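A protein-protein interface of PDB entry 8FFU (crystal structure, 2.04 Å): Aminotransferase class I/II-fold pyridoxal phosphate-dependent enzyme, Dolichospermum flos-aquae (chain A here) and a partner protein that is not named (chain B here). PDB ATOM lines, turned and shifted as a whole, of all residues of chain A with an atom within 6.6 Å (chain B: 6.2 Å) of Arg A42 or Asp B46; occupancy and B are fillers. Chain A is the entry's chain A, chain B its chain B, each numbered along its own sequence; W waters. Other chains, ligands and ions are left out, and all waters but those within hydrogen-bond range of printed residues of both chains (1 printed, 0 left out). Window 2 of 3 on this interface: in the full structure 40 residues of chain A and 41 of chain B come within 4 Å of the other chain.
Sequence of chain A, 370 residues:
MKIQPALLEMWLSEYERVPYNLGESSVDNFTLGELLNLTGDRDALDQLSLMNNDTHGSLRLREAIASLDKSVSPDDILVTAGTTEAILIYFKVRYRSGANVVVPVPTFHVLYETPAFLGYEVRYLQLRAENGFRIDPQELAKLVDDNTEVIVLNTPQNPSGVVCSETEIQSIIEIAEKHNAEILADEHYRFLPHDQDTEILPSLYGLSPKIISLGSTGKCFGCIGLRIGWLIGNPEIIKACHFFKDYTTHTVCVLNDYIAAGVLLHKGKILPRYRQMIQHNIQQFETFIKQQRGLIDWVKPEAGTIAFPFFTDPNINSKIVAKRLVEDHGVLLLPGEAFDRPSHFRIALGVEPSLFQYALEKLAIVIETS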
ATOM      1  N   THR A  31     -10.160   7.367  21.181  1.00  0.00           N
ATOM      2  CA  THR A  31     -10.975   7.779  22.307  1.00  0.00           C
ATOM      3  C   THR A  31     -12.437   7.782  21.886  1.00  0.00           C
ATOM      4  O   THR A  31     -12.769   7.719  20.699  1.00  0.00           O
ATOM      5  CB  THR A  31     -10.576   9.166  22.814  1.00  0.00           C
ATOM      6  OG1 THR A  31     -10.943  10.151  21.845  1.00  0.00           O
ATOM      7  CG2 THR A  31      -9.079   9.246  23.087  1.00  0.00           C
ATOM      8  N   LEU A  32     -13.325   7.860  22.876  1.00  0.00           N
ATOM      9  CA  LEU A  32     -14.748   7.870  22.562  1.00  0.00           C
ATOM     10  C   LEU A  32     -15.111   9.089  21.725  1.00  0.00           C
ATOM     11  O   LEU A  32     -15.915   8.992  20.793  1.00  0.00           O
ATOM     12  CB  LEU A  32     -15.574   7.841  23.844  1.00  0.00           C
ATOM     13  CG  LEU A  32     -17.074   7.821  23.567  1.00  0.00           C
ATOM     14  CD1 LEU A  32     -17.451   6.500  22.916  1.00  0.00           C
ATOM     15  CD2 LEU A  32     -17.885   8.056  24.827  1.00  0.00           C
ATOM     16  N   GLY A  33     -14.518  10.243  22.038  1.00  0.00           N
ATOM     17  CA  GLY A  33     -14.810  11.447  21.278  1.00  0.00           C
ATOM     18  C   GLY A  33     -14.318  11.374  19.845  1.00  0.00           C
ATOM     19  O   GLY A  33     -14.996  11.835  18.923  1.00  0.00           O
ATOM     20  N   GLU A  34     -13.130  10.804  19.640  1.00  0.00           N
ATOM     21  CA  GLU A  34     -12.602  10.647  18.289  1.00  0.00           C
ATOM     22  C   GLU A  34     -13.507   9.755  17.449  1.00  0.00           C
ATOM     23  O   GLU A  34     -13.858  10.098  16.314  1.00  0.00           O
ATOM     24  CB  GLU A  34     -11.194  10.062  18.356  1.00  0.00           C
ATOM     25  CG  GLU A  34     -10.141  11.028  18.837  1.00  0.00           C
ATOM     26  CD  GLU A  34      -8.902  10.311  19.310  1.00  0.00           C
ATOM     27  OE1 GLU A  34      -8.947   9.070  19.416  1.00  0.00           O
ATOM     28  OE2 GLU A  34      -7.886  10.979  19.577  1.00  0.00           O
ATOM     29  N   LEU A  35     -13.925   8.618  18.009  1.00  0.00           N
ATOM     30  CA  LEU A  35     -14.757   7.684  17.259  1.00  0.00           C
ATOM     31  C   LEU A  35     -16.127   8.282  16.950  1.00  0.00           C
ATOM     32  O   LEU A  35     -16.658   8.090  15.851  1.00  0.00           O
ATOM     33  CB  LEU A  35     -14.892   6.376  18.034  1.00  0.00           C
ATOM     34  CG  LEU A  35     -15.637   5.215  17.377  1.00  0.00           C
ATOM     35  CD1 LEU A  35     -14.953   4.799  16.089  1.00  0.00           C
ATOM     36  CD2 LEU A  35     -15.723   4.047  18.330  1.00  0.00           C
ATOM     37  N   LEU A  36     -16.709   9.022  17.899  1.00  0.00           N
ATOM     38  CA  LEU A  36     -18.026   9.610  17.662  1.00  0.00           C
ATOM     39  C   LEU A  36     -17.968  10.717  16.621  1.00  0.00           C
ATOM     40  O   LEU A  36     -18.973  10.991  15.960  1.00  0.00           O
ATOM     41  CB  LEU A  36     -18.617  10.145  18.968  1.00  0.00           C
ATOM     42  CG  LEU A  36     -19.067   9.103  19.991  1.00  0.00           C
ATOM     43  CD1 LEU A  36     -19.559   9.783  21.263  1.00  0.00           C
ATOM     44  CD2 LEU A  36     -20.148   8.220  19.400  1.00  0.00           C
ATOM     45  N   ASN A  37     -16.823  11.382  16.480  1.00  0.00           N
ATOM     46  CA  ASN A  37     -16.675  12.367  15.416  1.00  0.00           C
ATOM     47  C   ASN A  37     -16.674  11.726  14.034  1.00  0.00           C
ATOM     48  O   ASN A  37     -16.949  12.414  13.045  1.00  0.00           O
ATOM     49  CB  ASN A  37     -15.398  13.181  15.623  1.00  0.00           C
ATOM     50  CG  ASN A  37     -15.451  14.036  16.877  1.00  0.00           C
ATOM     51  OD1 ASN A  37     -16.527  14.434  17.321  1.00  0.00           O
ATOM     52  ND2 ASN A  37     -14.289  14.323  17.454  1.00  0.00           N
ATOM     53  N   THR A  39     -18.426   8.537  13.453  1.00  0.00           N
ATOM     54  CA  THR A  39     -19.695   7.848  13.272  1.00  0.00           C
ATOM     55  C   THR A  39     -20.907   8.760  13.407  1.00  0.00           C
ATOM     56  O   THR A  39     -21.980   8.415  12.898  1.00  0.00           O
ATOM     57  CB  THR A  39     -19.820   6.691  14.268  1.00  0.00           C
ATOM     58  OG1 THR A  39     -19.965   7.210  15.596  1.00  0.00           O
ATOM     59  CG2 THR A  39     -18.587   5.799  14.207  1.00  0.00           C
ATOM     60  N   GLY A  40     -20.773   9.904  14.078  1.00  0.00           N
ATOM     61  CA  GLY A  40     -21.893  10.814  14.209  1.00  0.00           C
ATOM     62  C   GLY A  40     -22.978  10.369  15.162  1.00  0.00           C
ATOM     63  O   GLY A  40     -24.092  10.890  15.097  1.00  0.00           O
ATOM     64  N   ASP A  41     -22.693   9.415  16.044  1.00  0.00           N
ATOM     65  CA  ASP A  41     -23.700   8.851  16.935  1.00  0.00           C
ATOM     66  C   ASP A  41     -23.816   9.580  18.276  1.00  0.00           C
ATOM     67  O   ASP A  41     -24.527   9.097  19.160  1.00  0.00           O
ATOM     68  CB  ASP A  41     -23.398   7.368  17.188  1.00  0.00           C
ATOM     69  CG  ASP A  41     -23.862   6.469  16.049  1.00  0.00           C
ATOM     70  OD1 ASP A  41     -24.615   6.948  15.182  1.00  0.00           O
ATOM     71  OD2 ASP A  41     -23.476   5.281  16.024  1.00  0.00           O
ATOM     72  N   ARG A  42     -23.153  10.727  18.451  1.00  0.00           N
ATOM     73  CA  ARG A  42     -23.071  11.335  19.779  1.00  0.00           C
ATOM     74  C   ARG A  42     -24.428  11.832  20.268  1.00  0.00           C
ATOM     75  O   ARG A  42     -24.853  11.499  21.380  1.00  0.00           O
ATOM     76  CB  ARG A  42     -22.051  12.476  19.780  1.00  0.00           C
ATOM     77  CG  ARG A  42     -21.929  13.195  21.122  1.00  0.00           C
ATOM     78  CD  ARG A  42     -20.907  14.328  21.078  1.00  0.00           C
ATOM     79  NE  ARG A  42     -19.535  13.843  21.198  1.00  0.00           N
ATOM     80  CZ  ARG A  42     -18.687  13.720  20.184  1.00  0.00           C
ATOM     81  NH1 ARG A  42     -19.034  14.045  18.949  1.00  0.00           N
ATOM     82  NH2 ARG A  42     -17.460  13.264  20.415  1.00  0.00           N
ATOM     83  N   ASP A  43     -25.126  12.630  19.454  1.00  0.00           N
ATOM     84  CA  ASP A  43     -26.367  13.251  19.913  1.00  0.00           C
ATOM     85  C   ASP A  43     -27.472  12.234  20.178  1.00  0.00           C
ATOM     86  O   ASP A  43     -28.433  12.551  20.886  1.00  0.00           O
ATOM     87  CB  ASP A  43     -26.840  14.308  18.909  1.00  0.00           C
ATOM     88  CG  ASP A  43     -26.988  13.764  17.500  1.00  0.00           C
ATOM     89  OD1 ASP A  43     -26.967  12.528  17.320  1.00  0.00           O
ATOM     90  OD2 ASP A  43     -27.121  14.585  16.563  1.00  0.00           O
ATOM     91  N   ALA A  44     -27.376  11.037  19.608  1.00  0.00           N
ATOM     92  CA  ALA A  44     -28.389  10.013  19.816  1.00  0.00           C
ATOM     93  C   ALA A  44     -28.191   9.233  21.108  1.00  0.00           C
ATOM     94  O   ALA A  44     -29.101   8.508  21.514  1.00  0.00           O
ATOM     95  CB  ALA A  44     -28.405   9.039  18.637  1.00  0.00           C
ATOM     96  N   LEU A  45     -27.025   9.351  21.748  1.00  0.00           N
ATOM     97  CA  LEU A  45     -26.708   8.495  22.890  1.00  0.00           C
ATOM     98  C   LEU A  45     -27.537   8.840  24.123  1.00  0.00           C
ATOM     99  O   LEU A  45     -27.930   7.945  24.876  1.00  0.00           O
ATOM    100  CB  LEU A  45     -25.221   8.599  23.221  1.00  0.00           C
ATOM    101  CG  LEU A  45     -24.228   8.051  22.196  1.00  0.00           C
ATOM    102  CD1 LEU A  45     -22.801   8.187  22.722  1.00  0.00           C
ATOM    103  CD2 LEU A  45     -24.553   6.606  21.857  1.00  0.00           C
ATOM    104  N   ASP A  46     -27.813  10.126  24.350  1.00  0.00           N
ATOM    105  CA  ASP A  46     -28.481  10.533  25.584  1.00  0.00           C
ATOM    106  C   ASP A  46     -29.922  10.054  25.669  1.00  0.00           C
ATOM    107  O   ASP A  46     -30.464   9.966  26.775  1.00  0.00           O
ATOM    108  CB  ASP A  46     -28.431  12.053  25.737  1.00  0.00           C
ATOM    109  CG  ASP A  46     -27.123  12.536  26.340  1.00  0.00           C
ATOM    110  OD1 ASP A  46     -26.257  11.688  26.655  1.00  0.00           O
ATOM    111  OD2 ASP A  46     -26.962  13.766  26.498  1.00  0.00           O
ATOM    112  N   GLN A  47     -30.557   9.755  24.542  1.00  0.00           N
ATOM    113  CA  GLN A  47     -31.925   9.257  24.535  1.00  0.00           C
ATOM    114  C   GLN A  47     -32.002   7.743  24.626  1.00  0.00           C
ATOM    115  O   GLN A  47     -33.107   7.193  24.590  1.00  0.00           O
ATOM    116  CB  GLN A  47     -32.653   9.745  23.285  1.00  0.00           C
ATOM    117  CG  GLN A  47     -33.017  11.215  23.354  1.00  0.00           C
ATOM    118  CD  GLN A  47     -31.832  12.119  23.080  1.00  0.00           C
ATOM    119  OE1 GLN A  47     -31.735  13.220  23.630  1.00  0.00           O
ATOM    120  NE2 GLN A  47     -30.915  11.656  22.232  1.00  0.00           N
ATOM    121  N   TYR A 258     -24.780   0.260  20.568  1.00  0.00           N
ATOM    122  CA  TYR A 258     -25.098   1.333  19.635  1.00  0.00           C
ATOM    123  C   TYR A 258     -23.839   1.925  19.016  1.00  0.00           C
ATOM    124  O   TYR A 258     -23.811   2.225  17.816  1.00  0.00           O
ATOM    125  CB  TYR A 258     -25.893   2.417  20.355  1.00  0.00           C
ATOM    126  CG  TYR A 258     -26.528   3.422  19.440  1.00  0.00           C
ATOM    127  CD1 TYR A 258     -27.797   3.210  18.931  1.00  0.00           C
ATOM    128  CD2 TYR A 258     -25.868   4.588  19.092  1.00  0.00           C
ATOM    129  CE1 TYR A 258     -28.390   4.127  18.097  1.00  0.00           C
ATOM    130  CE2 TYR A 258     -26.452   5.511  18.255  1.00  0.00           C
ATOM    131  CZ  TYR A 258     -27.712   5.273  17.758  1.00  0.00           C
ATOM    132  OH  TYR A 258     -28.304   6.189  16.923  1.00  0.00           O
ATOM    133  N   ARG B  42     -20.727  13.516  32.025  1.00  0.00           N
ATOM    134  CA  ARG B  42     -20.915  13.487  30.572  1.00  0.00           C
ATOM    135  C   ARG B  42     -19.665  13.943  29.824  1.00  0.00           C
ATOM    136  O   ARG B  42     -19.172  13.244  28.934  1.00  0.00           O
ATOM    137  CB  ARG B  42     -22.106  14.363  30.175  1.00  0.00           C
ATOM    138  CG  ARG B  42     -22.335  14.449  28.667  1.00  0.00           C
ATOM    139  CD  ARG B  42     -23.503  15.366  28.300  1.00  0.00           C
ATOM    140  NE  ARG B  42     -24.810  14.735  28.449  1.00  0.00           N
ATOM    141  CZ  ARG B  42     -25.629  14.956  29.468  1.00  0.00           C
ATOM    142  NH1 ARG B  42     -25.302  15.783  30.444  1.00  0.00           N
ATOM    143  NH2 ARG B  42     -26.807  14.338  29.503  1.00  0.00           N
ATOM    144  N   ASP B  43     -19.137  15.115  30.172  1.00  0.00           N
ATOM    145  CA  ASP B  43     -18.029  15.687  29.415  1.00  0.00           C
ATOM    146  C   ASP B  43     -16.745  14.881  29.538  1.00  0.00           C
ATOM    147  O   ASP B  43     -15.866  15.009  28.678  1.00  0.00           O
ATOM    148  CB  ASP B  43     -17.799  17.130  29.848  1.00  0.00           C
ATOM    149  CG  ASP B  43     -18.940  18.044  29.430  1.00  0.00           C
ATOM    150  OD1 ASP B  43     -19.686  17.665  28.501  1.00  0.00           O
ATOM    151  OD2 ASP B  43     -19.095  19.131  30.028  1.00  0.00           O
ATOM    152  N   ALA B  44     -16.620  14.047  30.572  1.00  0.00           N
ATOM    153  CA  ALA B  44     -15.401  13.277  30.777  1.00  0.00           C
ATOM    154  C   ALA B  44     -15.341  12.026  29.916  1.00  0.00           C
ATOM    155  O   ALA B  44     -14.260  11.446  29.769  1.00  0.00           O
ATOM    156  CB  ALA B  44     -15.270  12.885  32.249  1.00  0.00           C
ATOM    157  N   LEU B  45     -16.469  11.608  29.342  1.00  0.00           N
ATOM    158  CA  LEU B  45     -16.517  10.345  28.614  1.00  0.00           C
ATOM    159  C   LEU B  45     -15.728  10.407  27.311  1.00  0.00           C
ATOM    160  O   LEU B  45     -15.158   9.398  26.889  1.00  0.00           O
ATOM    161  CB  LEU B  45     -17.969   9.952  28.334  1.00  0.00           C
ATOM    162  CG  LEU B  45     -18.849   9.583  29.529  1.00  0.00           C
ATOM    163  CD1 LEU B  45     -20.240   9.183  29.054  1.00  0.00           C
ATOM    164  CD2 LEU B  45     -18.221   8.465  30.345  1.00  0.00           C
ATOM    165  N   ASP B  46     -15.706  11.567  26.652  1.00  0.00           N
ATOM    166  CA  ASP B  46     -15.066  11.670  25.345  1.00  0.00           C
ATOM    167  C   ASP B  46     -13.546  11.525  25.400  1.00  0.00           C
ATOM    168  O   ASP B  46     -12.946  11.146  24.390  1.00  0.00           O
ATOM    169  CB  ASP B  46     -15.451  12.994  24.681  1.00  0.00           C
ATOM    170  CG  ASP B  46     -16.800  12.924  23.978  1.00  0.00           C
ATOM    171  OD1 ASP B  46     -17.427  11.844  24.003  1.00  0.00           O
ATOM    172  OD2 ASP B  46     -17.234  13.935  23.392  1.00  0.00           O
ATOM    173  N   GLN B  47     -12.909  11.792  26.538  1.00  0.00           N
ATOM    174  CA  GLN B  47     -11.463  11.613  26.647  1.00  0.00           C
ATOM    175  C   GLN B  47     -11.067  10.203  27.050  1.00  0.00           C
ATOM    176  O   GLN B  47      -9.872   9.934  27.207  1.00  0.00           O
ATOM    177  CB  GLN B  47     -10.846  12.603  27.647  1.00  0.00           C
ATOM    178  CG  GLN B  47     -10.676  14.015  27.132  1.00  0.00           C
ATOM    179  CD  GLN B  47     -11.951  14.808  27.149  1.00  0.00           C
ATOM    180  OE1 GLN B  47     -12.165  15.676  26.301  1.00  0.00           O
ATOM    181  NE2 GLN B  47     -12.812  14.527  28.122  1.00  0.00           N
ATOM    182  N   LEU B  48     -12.029   9.310  27.248  1.00  0.00           N
ATOM    183  CA  LEU B  48     -11.712   7.944  27.630  1.00  0.00           C
ATOM    184  C   LEU B  48     -11.210   7.162  26.423  1.00  0.00           C
ATOM    185  O   LEU B  48     -11.797   7.225  25.340  1.00  0.00           O
ATOM    186  CB  LEU B  48     -12.935   7.269  28.247  1.00  0.00           C
ATOM    187  CG  LEU B  48     -13.317   7.864  29.600  1.00  0.00           C
ATOM    188  CD1 LEU B  48     -14.540   7.175  30.170  1.00  0.00           C
ATOM    189  CD2 LEU B  48     -12.140   7.739  30.548  1.00  0.00           C
ATOM    190  N   SER B  49     -10.113   6.438  26.616  1.00  0.00           N
ATOM    191  CA  SER B  49      -9.544   5.610  25.566  1.00  0.00           C
ATOM    192  C   SER B  49     -10.318   4.301  25.476  1.00  0.00           C
ATOM    193  O   SER B  49     -10.719   3.731  26.492  1.00  0.00           O
ATOM    194  CB  SER B  49      -8.064   5.341  25.850  1.00  0.00           C
ATOM    195  OG  SER B  49      -7.537   4.364  24.972  1.00  0.00           O
ATOM    196  N   LEU B 255     -16.141   2.648  29.536  1.00  0.00           N
ATOM    197  CA  LEU B 255     -17.221   3.627  29.561  1.00  0.00           C
ATOM    198  C   LEU B 255     -18.262   3.263  30.613  1.00  0.00           C
ATOM    199  O   LEU B 255     -18.609   4.088  31.464  1.00  0.00           O
ATOM    200  CB  LEU B 255     -17.865   3.719  28.177  1.00  0.00           C
ATOM    201  CG  LEU B 255     -16.951   4.173  27.030  1.00  0.00           C
ATOM    202  CD1 LEU B 255     -17.676   4.098  25.689  1.00  0.00           C
ATOM    203  CD2 LEU B 255     -16.389   5.572  27.266  1.00  0.00           C
HETATM  204  O   HOH W   1     -29.701  14.377  28.382  1.00  0.00           O
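Printed residues of chain B that touch a printed residue of chain A: Arg B42, Leu B45, Asp B46, Leu B48 and Leu B255.
Hydrophobic or aromatic side chains of chain B that line the printed part of chain A: Leu B45 and Leu B255.
Of the 17 printed residues of chain A, 5 touch a printed residue of chain B.
Hydrophobic or aromatic side chains of chain A that line the printed part of chain B: Leu A32.
Among the printed residues, Asp or Glu carboxylates within 4 Å of a Lys or Arg side-chain nitrogen of the other chain: Arg A42 with Asp B46 (3.1 Å) and Asp A46 with Arg B42 (3.1 Å).
Of the printed residues of chain B, Thr A31 touches Asp B46 (3.4 Å) and Leu B48 (3.2 Å).
Gly A40 touches none of the printed residues of chain B.
Of the printed residues of chain B, Asp A46 touches Arg B42.
Of chain A, only Thr A31, Leu A32, Gly A33 and Arg A42 come within 4 Å of Asp B46.
The nearest printed residue of chain A that does not touch Leu B255 is Thr A31 (7.0 Å).
N of Leu A32 is in hydrogen-bond range of O of Leu B48 (3.0 Å).
The guanidinium group of Arg A42 is in salt-bridge range of the side-chain carboxylate of Asp B46 (3.1 Å).
OG1 of Thr A31 lies within hydrogen-bond range of O of Asp B46 (3.4 Å).
N of Gly A33 sits at hydrogen-bond distance from O of Asp B46, at 3.0 Å.
The side-chain carboxylate of Asp A46 lies within salt-bridge range of the guanidinium group of Arg B42, 3.1 Å away.
The side-chain amide oxygen (OD1) of Asn A37 is in hydrogen-bond range of the guanidinium group (NH1) of Arg A42.
O of Gly A33 sits at hydrogen-bond distance from NH2 of Arg A42, at 3.2 Å.
OE1 of Glu A34 lies within hydrogen-bond range of N of Thr A31 (2.7 Å).
The side-chain amide nitrogen of Asn A37 is in hydrogen-bond range of the backbone carbonyl oxygen of Gly A33, at 3.0 Å.
Among the printed residues, pairs that only touch across the chains: Thr A31 with Leu B48 (3.2 Å), Leu A32 with Leu B45 (3.4 Å), Leu A32 with Asp B46 (3.6 Å) and Leu A32 with Leu B255 (3.7 Å).
Water W1 bridges NH2 of Arg B42 and OD2 of Asp A46.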
